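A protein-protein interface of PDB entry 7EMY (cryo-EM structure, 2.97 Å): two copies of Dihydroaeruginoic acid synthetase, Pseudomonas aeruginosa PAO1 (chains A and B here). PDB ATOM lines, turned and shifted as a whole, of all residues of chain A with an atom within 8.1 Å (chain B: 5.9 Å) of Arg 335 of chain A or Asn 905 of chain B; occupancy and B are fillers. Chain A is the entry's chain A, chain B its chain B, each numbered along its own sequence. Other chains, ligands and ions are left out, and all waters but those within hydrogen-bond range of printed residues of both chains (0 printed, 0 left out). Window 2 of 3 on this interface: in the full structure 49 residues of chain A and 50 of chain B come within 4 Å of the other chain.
NH2 of Arg 332 of chain A is in salt-bridge range of OE1 of Glu 708 of chain B, 3.2 Å away.
O of Arg 904 of chain B is in hydrogen-bond range of NE of Arg 332 of chain A, at 3.5 Å.
The side-chain carboxylate (OE1) of Glu 708 of chain B sits close to the side-chain carboxylate (OD2) of Asp 522 of chain A (3.1 Å).
NE of Arg 332 of chain A sits close to O of Cys 521 of chain A (3.3 Å).
The side-chain carboxylate (OD1) of Asp 522 of chain A is in salt-bridge range of the guanidinium group (NH2) of Arg 332 of chain A, 2.8 Å away.
The backbone carbonyl oxygen (O) of Ala 649 of chain B sits at hydrogen-bond distance from the side-chain amide nitrogen (ND2) of Asn 905 of chain B, 2.5 Å away.
The backbone carbonyl oxygen (O) of Ala 650 of chain B sits at hydrogen-bond distance from the guanidinium group (NE) of Arg 904 of chain B, 3.0 Å away.
O of Ala 650 of chain B sits close to ND2 of Asn 905 of chain B (3.3 Å).
OE2 of Glu 708 of chain B lies within salt-bridge range of NH1 of Arg 904 of chain B, at 2.7 Å.
CD of Arg 332 of chain A touches OD1 of Asn 905 of chain B, 3.5 Å away.
Asn 905 of chain B touches Arg 335 of chain A.
O of Tyr 903 of chain B touches O of Asp 522 of chain A, 3.7 Å away.
O of Asp 522 of chain A touches CA of Pro 907 of chain B, at 3.9 Å.
Pro 907 of chain B touches Ser 523 of chain A (CB to C, 3.6 Å).
Of the printed residues of chain B, Arg 332 of chain A touches Glu 708, Arg 904 and Asn 905.
Arg 335 of chain A touches just one residue of chain B: Asn 905 (3.9 Å).
Of the printed residues of chain B, Ser 523 of chain A touches Pro 907 (3.6 Å).
Printed residues of chain A within 4 Å of Tyr 903 of chain B: Asp 522 (3.7 Å).
Of the printed residues of chain A, Arg 904 of chain B touches Arg 332 (3.4 Å).
Printed residues of chain A within 4 Å of Pro 907 of chain B: Asp 522 and Ser 523.
The nearest printed residue of chain A that does not touch Pro 907 of chain B is Leu 336 of chain A (4.5 Å).
Of the 13 printed residues of chain B, 5 touch a printed residue of chain A.
Of the 24 printed residues of chain A, 4 touch a printed residue of chain B.
Along chain A the printed residues that touch a printed residue of chain B span positions 332 to 523.
Among the printed residues, Asp or Glu carboxylates within 4 Å of a Lys or Arg side-chain nitrogen of the other chain: Arg 332 of chain A with Glu 708 of chain B.
No position is printed for both chains.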
ATOM      1  N   LEU A  40      -5.223  12.869   3.851  1.00  0.00           N
ATOM      2  CA  LEU A  40      -4.285  11.766   4.068  1.00  0.00           C
ATOM      3  C   LEU A  40      -4.989  10.446   3.730  1.00  0.00           C
ATOM      4  O   LEU A  40      -4.407   9.559   3.114  1.00  0.00           O
ATOM      5  CB  LEU A  40      -3.763  11.765   5.512  1.00  0.00           C
ATOM      6  CG  LEU A  40      -3.506  13.153   6.119  1.00  0.00           C
ATOM      7  CD1 LEU A  40      -2.913  13.013   7.512  1.00  0.00           C
ATOM      8  CD2 LEU A  40      -2.557  14.025   5.306  1.00  0.00           C
ATOM      9  N   GLY A  41      -6.294  10.386   3.990  1.00  0.00           N
ATOM     10  CA  GLY A  41      -7.248   9.442   3.412  1.00  0.00           C
ATOM     11  C   GLY A  41      -7.304   9.420   1.879  1.00  0.00           C
ATOM     12  O   GLY A  41      -7.874   8.504   1.305  1.00  0.00           O
ATOM     13  N   ALA A 327       5.522  -4.615  -2.663  1.00  0.00           N
ATOM     14  CA  ALA A 327       4.553  -3.696  -3.244  1.00  0.00           C
ATOM     15  C   ALA A 327       3.188  -3.876  -2.598  1.00  0.00           C
ATOM     16  O   ALA A 327       2.506  -2.897  -2.282  1.00  0.00           O
ATOM     17  CB  ALA A 327       4.470  -3.912  -4.754  1.00  0.00           C
ATOM     18  N   GLY A 328       2.776  -5.126  -2.385  1.00  0.00           N
ATOM     19  CA  GLY A 328       1.509  -5.368  -1.715  1.00  0.00           C
ATOM     20  C   GLY A 328       1.500  -4.850  -0.291  1.00  0.00           C
ATOM     21  O   GLY A 328       0.515  -4.258   0.160  1.00  0.00           O
ATOM     22  N   GLU A 329       2.535  -5.028   0.462  1.00  0.00           N
ATOM     23  CA  GLU A 329       2.735  -4.536   1.770  1.00  0.00           C
ATOM     24  C   GLU A 329       2.630  -3.035   1.821  1.00  0.00           C
ATOM     25  O   GLU A 329       1.961  -2.438   2.674  1.00  0.00           O
ATOM     26  CB  GLU A 329       3.908  -5.105   2.447  1.00  0.00           C
ATOM     27  CG  GLU A 329       3.968  -6.459   2.925  1.00  0.00           C
ATOM     28  CD  GLU A 329       5.246  -7.054   3.355  1.00  0.00           C
ATOM     29  OE1 GLU A 329       6.279  -6.530   2.889  1.00  0.00           O
ATOM     30  OE2 GLU A 329       5.271  -8.012   4.155  1.00  0.00           O
ATOM     31  N   SER A 330       3.283  -2.355   0.938  1.00  0.00           N
ATOM     32  CA  SER A 330       3.267  -0.955   0.753  1.00  0.00           C
ATOM     33  C   SER A 330       1.872  -0.448   0.497  1.00  0.00           C
ATOM     34  O   SER A 330       1.391   0.521   1.094  1.00  0.00           O
ATOM     35  CB  SER A 330       4.219  -0.393  -0.212  1.00  0.00           C
ATOM     36  OG  SER A 330       4.285   0.952  -0.355  1.00  0.00           O
ATOM     37  N   ARG A 331       1.167  -1.057  -0.399  1.00  0.00           N
ATOM     38  CA  ARG A 331      -0.172  -0.793  -0.757  1.00  0.00           C
ATOM     39  C   ARG A 331      -1.086  -0.869   0.434  1.00  0.00           C
ATOM     40  O   ARG A 331      -1.930  -0.004   0.687  1.00  0.00           O
ATOM     41  CB  ARG A 331      -0.643  -1.535  -1.936  1.00  0.00           C
ATOM     42  CG  ARG A 331      -0.085  -1.290  -3.234  1.00  0.00           C
ATOM     43  CD  ARG A 331       0.022   0.081  -3.622  1.00  0.00           C
ATOM     44  NE  ARG A 331       1.166   0.751  -3.236  1.00  0.00           N
ATOM     45  CZ  ARG A 331       2.360   0.670  -3.726  1.00  0.00           C
ATOM     46  NH1 ARG A 331       2.539  -0.017  -4.724  1.00  0.00           N
ATOM     47  NH2 ARG A 331       3.314   1.266  -3.224  1.00  0.00           N
ATOM     48  N   ARG A 332      -0.991  -1.905   1.198  1.00  0.00           N
ATOM     49  CA  ARG A 332      -1.742  -2.173   2.361  1.00  0.00           C
ATOM     50  C   ARG A 332      -1.521  -1.136   3.428  1.00  0.00           C
ATOM     51  O   ARG A 332      -2.452  -0.632   4.067  1.00  0.00           O
ATOM     52  CB  ARG A 332      -1.660  -3.566   2.812  1.00  0.00           C
ATOM     53  CG  ARG A 332      -2.191  -4.650   2.044  1.00  0.00           C
ATOM     54  CD  ARG A 332      -2.506  -5.884   2.689  1.00  0.00           C
ATOM     55  NE  ARG A 332      -1.451  -6.721   2.989  1.00  0.00           N
ATOM     56  CZ  ARG A 332      -0.767  -7.489   2.207  1.00  0.00           C
ATOM     57  NH1 ARG A 332      -1.056  -7.522   1.018  1.00  0.00           N
ATOM     58  NH2 ARG A 332       0.158  -8.186   2.619  1.00  0.00           N
ATOM     59  N   LEU A 333      -0.307  -0.773   3.686  1.00  0.00           N
ATOM     60  CA  LEU A 333       0.090   0.257   4.565  1.00  0.00           C
ATOM     61  C   LEU A 333      -0.525   1.574   4.189  1.00  0.00           C
ATOM     62  O   LEU A 333      -1.083   2.307   5.011  1.00  0.00           O
ATOM     63  CB  LEU A 333       1.531   0.312   4.840  1.00  0.00           C
ATOM     64  CG  LEU A 333       2.231  -0.625   5.726  1.00  0.00           C
ATOM     65  CD1 LEU A 333       3.627  -0.469   5.781  1.00  0.00           C
ATOM     66  CD2 LEU A 333       1.640  -0.674   7.008  1.00  0.00           C
ATOM     67  N   GLU A 334      -0.447   1.947   2.955  1.00  0.00           N
ATOM     68  CA  GLU A 334      -1.014   3.104   2.382  1.00  0.00           C
ATOM     69  C   GLU A 334      -2.501   3.163   2.603  1.00  0.00           C
ATOM     70  O   GLU A 334      -3.070   4.160   3.062  1.00  0.00           O
ATOM     71  CB  GLU A 334      -0.577   3.347   1.004  1.00  0.00           C
ATOM     72  CG  GLU A 334       0.792   3.573   0.643  1.00  0.00           C
ATOM     73  CD  GLU A 334       1.229   3.492  -0.762  1.00  0.00           C
ATOM     74  OE1 GLU A 334       0.456   2.900  -1.545  1.00  0.00           O
ATOM     75  OE2 GLU A 334       2.304   4.009  -1.129  1.00  0.00           O
ATOM     76  N   ARG A 335      -3.197   2.118   2.296  1.00  0.00           N
ATOM     77  CA  ARG A 335      -4.592   1.946   2.432  1.00  0.00           C
ATOM     78  C   ARG A 335      -5.044   2.126   3.856  1.00  0.00           C
ATOM     79  O   ARG A 335      -6.007   2.834   4.164  1.00  0.00           O
ATOM     80  CB  ARG A 335      -5.116   0.746   1.767  1.00  0.00           C
ATOM     81  CG  ARG A 335      -5.166   0.584   0.346  1.00  0.00           C
ATOM     82  CD  ARG A 335      -6.071  -0.387  -0.192  1.00  0.00           C
ATOM     83  NE  ARG A 335      -5.851  -1.714   0.129  1.00  0.00           N
ATOM     84  CZ  ARG A 335      -5.202  -2.639  -0.501  1.00  0.00           C
ATOM     85  NH1 ARG A 335      -4.728  -2.378  -1.602  1.00  0.00           N
ATOM     86  NH2 ARG A 335      -5.052  -3.771  -0.036  1.00  0.00           N
ATOM     87  N   LEU A 336      -4.405   1.490   4.781  1.00  0.00           N
ATOM     88  CA  LEU A 336      -4.670   1.509   6.168  1.00  0.00           C
ATOM     89  C   LEU A 336      -4.428   2.864   6.775  1.00  0.00           C
ATOM     90  O   LEU A 336      -5.190   3.362   7.610  1.00  0.00           O
ATOM     91  CB  LEU A 336      -4.089   0.379   6.898  1.00  0.00           C
ATOM     92  CG  LEU A 336      -4.625  -0.985   6.794  1.00  0.00           C
ATOM     93  CD1 LEU A 336      -3.737  -2.011   7.156  1.00  0.00           C
ATOM     94  CD2 LEU A 336      -5.877  -1.111   7.440  1.00  0.00           C
ATOM     95  N   ALA A 337      -3.325   3.485   6.343  1.00  0.00           N
ATOM     96  CA  ALA A 337      -2.960   4.851   6.674  1.00  0.00           C
ATOM     97  C   ALA A 337      -4.051   5.805   6.210  1.00  0.00           C
ATOM     98  O   ALA A 337      -4.509   6.647   6.969  1.00  0.00           O
ATOM     99  CB  ALA A 337      -1.633   5.208   5.999  1.00  0.00           C
ATOM    100  N   ALA A 338      -4.531   5.627   4.984  1.00  0.00           N
ATOM    101  CA  ALA A 338      -5.645   6.386   4.475  1.00  0.00           C
ATOM    102  C   ALA A 338      -6.909   6.165   5.329  1.00  0.00           C
ATOM    103  O   ALA A 338      -7.520   7.129   5.768  1.00  0.00           O
ATOM    104  CB  ALA A 338      -5.829   6.017   3.000  1.00  0.00           C
ATOM    105  N   GLN A 339      -7.273   4.925   5.651  1.00  0.00           N
ATOM    106  CA  GLN A 339      -8.464   4.622   6.455  1.00  0.00           C
ATOM    107  C   GLN A 339      -8.433   5.240   7.853  1.00  0.00           C
ATOM    108  O   GLN A 339      -9.439   5.739   8.348  1.00  0.00           O
ATOM    109  CB  GLN A 339      -8.618   3.108   6.600  1.00  0.00           C
ATOM    110  CG  GLN A 339      -9.084   2.441   5.307  1.00  0.00           C
ATOM    111  CD  GLN A 339      -8.951   0.926   5.358  1.00  0.00           C
ATOM    112  OE1 GLN A 339      -9.034   0.291   6.397  1.00  0.00           O
ATOM    113  NE2 GLN A 339      -8.751   0.279   4.237  1.00  0.00           N
ATOM    114  N   HIS A 340      -7.272   5.240   8.492  1.00  0.00           N
ATOM    115  CA  HIS A 340      -6.951   5.801   9.746  1.00  0.00           C
ATOM    116  C   HIS A 340      -6.563   7.255   9.694  1.00  0.00           C
ATOM    117  O   HIS A 340      -6.289   7.865  10.733  1.00  0.00           O
ATOM    118  CB  HIS A 340      -6.050   4.950  10.537  1.00  0.00           C
ATOM    119  CG  HIS A 340      -6.418   3.574  10.836  1.00  0.00           C
ATOM    120  ND1 HIS A 340      -7.347   3.262  11.805  1.00  0.00           N
ATOM    121  CD2 HIS A 340      -6.112   2.409  10.320  1.00  0.00           C
ATOM    122  CE1 HIS A 340      -7.496   1.992  11.774  1.00  0.00           C
ATOM    123  NE2 HIS A 340      -6.778   1.483  10.911  1.00  0.00           N
ATOM    124  N   GLY A 341      -6.597   7.886   8.525  1.00  0.00           N
ATOM    125  CA  GLY A 341      -6.400   9.325   8.398  1.00  0.00           C
ATOM    126  C   GLY A 341      -4.998   9.772   8.798  1.00  0.00           C
ATOM    127  O   GLY A 341      -4.843  10.771   9.500  1.00  0.00           O
ATOM    128  N   VAL A 342      -3.970   9.019   8.406  1.00  0.00           N
ATOM    129  CA  VAL A 342      -2.572   9.351   8.682  1.00  0.00           C
ATOM    130  C   VAL A 342      -1.688   9.297   7.452  1.00  0.00           C
ATOM    131  O   VAL A 342      -1.948   8.552   6.512  1.00  0.00           O
ATOM    132  CB  VAL A 342      -1.942   8.518   9.804  1.00  0.00           C
ATOM    133  CG1 VAL A 342      -2.649   8.710  11.140  1.00  0.00           C
ATOM    134  CG2 VAL A 342      -1.918   7.035   9.493  1.00  0.00           C
ATOM    135  N   LEU A 344       1.644   8.086   5.579  1.00  0.00           N
ATOM    136  CA  LEU A 344       2.415   6.856   5.630  1.00  0.00           C
ATOM    137  C   LEU A 344       3.722   7.038   6.410  1.00  0.00           C
ATOM    138  O   LEU A 344       4.156   6.156   7.138  1.00  0.00           O
ATOM    139  CB  LEU A 344       2.670   6.440   4.185  1.00  0.00           C
ATOM    140  CG  LEU A 344       3.428   5.126   4.093  1.00  0.00           C
ATOM    141  CD1 LEU A 344       2.602   3.948   4.594  1.00  0.00           C
ATOM    142  CD2 LEU A 344       3.804   4.883   2.645  1.00  0.00           C
ATOM    143  N   LEU A 520       0.820  -4.614  10.658  1.00  0.00           N
ATOM    144  CA  LEU A 520       0.098  -3.499  10.193  1.00  0.00           C
ATOM    145  C   LEU A 520      -0.436  -3.709   8.803  1.00  0.00           C
ATOM    146  O   LEU A 520      -1.591  -3.397   8.494  1.00  0.00           O
ATOM    147  CB  LEU A 520       0.795  -2.225  10.402  1.00  0.00           C
ATOM    148  CG  LEU A 520       1.218  -1.768  11.733  1.00  0.00           C
ATOM    149  CD1 LEU A 520       2.149  -0.712  11.756  1.00  0.00           C
ATOM    150  CD2 LEU A 520       0.114  -1.528  12.573  1.00  0.00           C
ATOM    151  N   CYS A 521       0.348  -4.226   7.917  1.00  0.00           N
ATOM    152  CA  CYS A 521       0.005  -4.613   6.603  1.00  0.00           C
ATOM    153  C   CYS A 521      -1.188  -5.528   6.596  1.00  0.00           C
ATOM    154  O   CYS A 521      -2.191  -5.320   5.903  1.00  0.00           O
ATOM    155  CB  CYS A 521       1.138  -5.096   5.798  1.00  0.00           C
ATOM    156  SG  CYS A 521       2.492  -4.115   5.349  1.00  0.00           S
ATOM    157  N   ASP A 522      -1.138  -6.580   7.342  1.00  0.00           N
ATOM    158  CA  ASP A 522      -1.984  -7.707   7.390  1.00  0.00           C
ATOM    159  C   ASP A 522      -3.004  -7.723   8.497  1.00  0.00           C
ATOM    160  O   ASP A 522      -3.722  -8.714   8.661  1.00  0.00           O
ATOM    161  CB  ASP A 522      -1.233  -8.962   7.247  1.00  0.00           C
ATOM    162  CG  ASP A 522      -0.291  -9.105   6.122  1.00  0.00           C
ATOM    163  OD1 ASP A 522      -0.207  -8.124   5.355  1.00  0.00           O
ATOM    164  OD2 ASP A 522       0.369 -10.153   5.961  1.00  0.00           O
ATOM    165  N   SER A 523      -3.106  -6.726   9.311  1.00  0.00           N
ATOM    166  CA  SER A 523      -3.942  -6.583  10.435  1.00  0.00           C
ATOM    167  C   SER A 523      -4.472  -5.190  10.627  1.00  0.00           C
ATOM    168  O   SER A 523      -3.766  -4.231  10.307  1.00  0.00           O
ATOM    169  CB  SER A 523      -3.424  -7.111  11.707  1.00  0.00           C
ATOM    170  OG  SER A 523      -4.316  -7.161  12.720  1.00  0.00           O
ATOM    171  N   TRP A 525      -5.365  -1.821  12.661  1.00  0.00           N
ATOM    172  CA  TRP A 525      -4.638  -1.006  13.553  1.00  0.00           C
ATOM    173  C   TRP A 525      -5.262  -0.861  14.914  1.00  0.00           C
ATOM    174  O   TRP A 525      -4.692  -0.205  15.793  1.00  0.00           O
ATOM    175  CB  TRP A 525      -4.193   0.251  12.940  1.00  0.00           C
ATOM    176  CG  TRP A 525      -3.375   0.198  11.738  1.00  0.00           C
ATOM    177  CD1 TRP A 525      -2.956  -0.891  11.115  1.00  0.00           C
ATOM    178  CD2 TRP A 525      -2.831   1.263  10.953  1.00  0.00           C
ATOM    179  NE1 TRP A 525      -2.246  -0.632  10.078  1.00  0.00           N
ATOM    180  CE2 TRP A 525      -2.112   0.676   9.894  1.00  0.00           C
ATOM    181  CE3 TRP A 525      -2.844   2.621  10.986  1.00  0.00           C
ATOM    182  CZ2 TRP A 525      -1.490   1.463   8.989  1.00  0.00           C
ATOM    183  CZ3 TRP A 525      -2.223   3.327  10.081  1.00  0.00           C
ATOM    184  CH2 TRP A 525      -1.556   2.744   9.096  1.00  0.00           C
ATOM    185  N   GLU B 648      -9.554 -12.070  -6.328  1.00  0.00           N
ATOM    186  CA  GLU B 648      -9.967 -10.792  -5.899  1.00  0.00           C
ATOM    187  C   GLU B 648      -9.508 -10.506  -4.494  1.00  0.00           C
ATOM    188  O   GLU B 648      -8.878  -9.487  -4.183  1.00  0.00           O
ATOM    189  CB  GLU B 648     -11.385 -10.447  -6.072  1.00  0.00           C
ATOM    190  CG  GLU B 648     -11.940  -9.180  -5.679  1.00  0.00           C
ATOM    191  CD  GLU B 648     -13.373  -8.897  -5.872  1.00  0.00           C
ATOM    192  OE1 GLU B 648     -14.045  -9.814  -6.387  1.00  0.00           O
ATOM    193  OE2 GLU B 648     -13.867  -7.801  -5.531  1.00  0.00           O
ATOM    194  N   ALA B 649      -9.802 -11.372  -3.581  1.00  0.00           N
ATOM    195  CA  ALA B 649      -9.419 -11.342  -2.225  1.00  0.00           C
ATOM    196  C   ALA B 649      -7.926 -11.299  -2.063  1.00  0.00           C
ATOM    197  O   ALA B 649      -7.364 -10.507  -1.299  1.00  0.00           O
ATOM    198  CB  ALA B 649     -10.023 -12.341  -1.408  1.00  0.00           C
ATOM    199  N   ALA B 650      -7.220 -12.136  -2.745  1.00  0.00           N
ATOM    200  CA  ALA B 650      -5.816 -12.268  -2.761  1.00  0.00           C
ATOM    201  C   ALA B 650      -5.105 -11.049  -3.279  1.00  0.00           C
ATOM    202  O   ALA B 650      -3.943 -10.799  -2.942  1.00  0.00           O
ATOM    203  CB  ALA B 650      -5.332 -13.451  -3.387  1.00  0.00           C
ATOM    204  N   GLY B 651      -5.707 -10.280  -4.118  1.00  0.00           N
ATOM    205  CA  GLY B 651      -5.078  -9.328  -4.882  1.00  0.00           C
ATOM    206  C   GLY B 651      -3.968  -9.846  -5.690  1.00  0.00           C
ATOM    207  O   GLY B 651      -2.887  -9.254  -5.793  1.00  0.00           O
ATOM    208  N   TYR B 696      -5.481 -20.487   0.764  1.00  0.00           N
ATOM    209  CA  TYR B 696      -6.869 -20.136   0.952  1.00  0.00           C
ATOM    210  C   TYR B 696      -7.591 -21.201   1.741  1.00  0.00           C
ATOM    211  O   TYR B 696      -8.024 -22.224   1.221  1.00  0.00           O
ATOM    212  CB  TYR B 696      -7.517 -19.806  -0.382  1.00  0.00           C
ATOM    213  CG  TYR B 696      -7.361 -18.334  -0.607  1.00  0.00           C
ATOM    214  CD1 TYR B 696      -6.144 -17.814  -1.055  1.00  0.00           C
ATOM    215  CD2 TYR B 696      -8.384 -17.475  -0.192  1.00  0.00           C
ATOM    216  CE1 TYR B 696      -5.952 -16.426  -1.079  1.00  0.00           C
ATOM    217  CE2 TYR B 696      -8.208 -16.086  -0.239  1.00  0.00           C
ATOM    218  CZ  TYR B 696      -6.970 -15.566  -0.642  1.00  0.00           C
ATOM    219  OH  TYR B 696      -6.722 -14.243  -0.509  1.00  0.00           O
ATOM    220  N   GLY B 706      -7.583 -16.064   2.756  1.00  0.00           N
ATOM    221  CA  GLY B 706      -6.255 -16.310   2.505  1.00  0.00           C
ATOM    222  C   GLY B 706      -5.287 -16.177   3.604  1.00  0.00           C
ATOM    223  O   GLY B 706      -5.120 -15.078   4.137  1.00  0.00           O
ATOM    224  N   GLU B 708      -1.857 -15.769   4.753  1.00  0.00           N
ATOM    225  CA  GLU B 708      -0.621 -15.225   4.330  1.00  0.00           C
ATOM    226  C   GLU B 708       0.479 -15.648   5.264  1.00  0.00           C
ATOM    227  O   GLU B 708       0.643 -15.024   6.314  1.00  0.00           O
ATOM    228  CB  GLU B 708      -0.581 -13.796   4.025  1.00  0.00           C
ATOM    229  CG  GLU B 708       0.492 -13.175   3.317  1.00  0.00           C
ATOM    230  CD  GLU B 708       0.356 -11.793   2.841  1.00  0.00           C
ATOM    231  OE1 GLU B 708      -0.645 -11.169   3.257  1.00  0.00           O
ATOM    232  OE2 GLU B 708       1.192 -11.293   2.061  1.00  0.00           O
ATOM    233  N   TYR B 903      -4.291 -12.794   7.568  1.00  0.00           N
ATOM    234  CA  TYR B 903      -4.972 -13.031   6.315  1.00  0.00           C
ATOM    235  C   TYR B 903      -4.594 -11.969   5.272  1.00  0.00           C
ATOM    236  O   TYR B 903      -4.323 -10.828   5.624  1.00  0.00           O
ATOM    237  CB  TYR B 903      -6.479 -13.144   6.533  1.00  0.00           C
ATOM    238  CG  TYR B 903      -6.892 -14.220   7.516  1.00  0.00           C
ATOM    239  CD1 TYR B 903      -6.896 -15.571   7.135  1.00  0.00           C
ATOM    240  CD2 TYR B 903      -7.293 -13.871   8.813  1.00  0.00           C
ATOM    241  CE1 TYR B 903      -7.315 -16.564   8.035  1.00  0.00           C
ATOM    242  CE2 TYR B 903      -7.679 -14.863   9.726  1.00  0.00           C
ATOM    243  CZ  TYR B 903      -7.692 -16.210   9.338  1.00  0.00           C
ATOM    244  OH  TYR B 903      -8.081 -17.160  10.216  1.00  0.00           O
ATOM    245  N   ARG B 904      -4.611 -12.317   3.981  1.00  0.00           N
ATOM    246  CA  ARG B 904      -4.082 -11.651   2.853  1.00  0.00           C
ATOM    247  C   ARG B 904      -4.583 -10.233   2.747  1.00  0.00           C
ATOM    248  O   ARG B 904      -3.828  -9.255   2.722  1.00  0.00           O
ATOM    249  CB  ARG B 904      -4.190 -12.344   1.561  1.00  0.00           C
ATOM    250  CG  ARG B 904      -3.700 -11.705   0.375  1.00  0.00           C
ATOM    251  CD  ARG B 904      -2.339 -11.259   0.330  1.00  0.00           C
ATOM    252  NE  ARG B 904      -1.814 -10.637  -0.792  1.00  0.00           N
ATOM    253  CZ  ARG B 904      -0.626 -10.233  -1.102  1.00  0.00           C
ATOM    254  NH1 ARG B 904       0.277 -10.380  -0.284  1.00  0.00           N
ATOM    255  NH2 ARG B 904      -0.378  -9.698  -2.187  1.00  0.00           N
ATOM    256  N   ASN B 905      -5.857 -10.048   2.674  1.00  0.00           N
ATOM    257  CA  ASN B 905      -6.587  -8.848   2.509  1.00  0.00           C
ATOM    258  C   ASN B 905      -7.800  -8.735   3.404  1.00  0.00           C
ATOM    259  O   ASN B 905      -8.852  -8.245   2.998  1.00  0.00           O
ATOM    260  CB  ASN B 905      -6.806  -8.538   1.093  1.00  0.00           C
ATOM    261  CG  ASN B 905      -5.643  -8.295   0.222  1.00  0.00           C
ATOM    262  OD1 ASN B 905      -4.708  -7.624   0.657  1.00  0.00           O
ATOM    263  ND2 ASN B 905      -5.629  -8.805  -0.896  1.00  0.00           N
ATOM    264  N   ASP B 906      -7.748  -9.200   4.607  1.00  0.00           N
ATOM    265  CA  ASP B 906      -8.716  -9.185   5.643  1.00  0.00           C
ATOM    266  C   ASP B 906      -8.145  -8.697   6.945  1.00  0.00           C
ATOM    267  O   ASP B 906      -8.053  -9.471   7.905  1.00  0.00           O
ATOM    268  CB  ASP B 906      -9.514 -10.409   5.802  1.00  0.00           C
ATOM    269  CG  ASP B 906     -10.783 -10.351   6.549  1.00  0.00           C
ATOM    270  OD1 ASP B 906     -10.853  -9.498   7.459  1.00  0.00           O
ATOM    271  OD2 ASP B 906     -11.735 -11.103   6.248  1.00  0.00           O
ATOM    272  N   PRO B 907      -7.708  -7.438   7.028  1.00  0.00           N
ATOM    273  CA  PRO B 907      -7.154  -6.933   8.270  1.00  0.00           C
ATOM    274  C   PRO B 907      -8.028  -7.088   9.476  1.00  0.00           C
ATOM    275  O   PRO B 907      -7.562  -7.366  10.588  1.00  0.00           O
ATOM    276  CB  PRO B 907      -6.779  -5.556   7.919  1.00  0.00           C
ATOM    277  CG  PRO B 907      -6.742  -5.469   6.533  1.00  0.00           C
ATOM    278  CD  PRO B 907      -7.655  -6.404   6.053  1.00  0.00           C
ATOM    279  N   GLU B 908      -9.299  -6.902   9.347  1.00  0.00           N
ATOM    280  CA  GLU B 908     -10.283  -6.999  10.354  1.00  0.00           C
ATOM    281  C   GLU B 908     -10.286  -8.360  10.997  1.00  0.00           C
ATOM    282  O   GLU B 908     -10.171  -8.530  12.217  1.00  0.00           O
ATOM    283  CB  GLU B 908     -11.601  -6.502   9.938  1.00  0.00           C
ATOM    284  CG  GLU B 908     -11.752  -5.161   9.444  1.00  0.00           C
ATOM    285  CD  GLU B 908     -11.264  -4.871   8.083  1.00  0.00           C
ATOM    286  OE1 GLU B 908     -10.752  -5.831   7.470  1.00  0.00           O
ATOM    287  OE2 GLU B 908     -11.369  -3.728   7.589  1.00  0.00           O
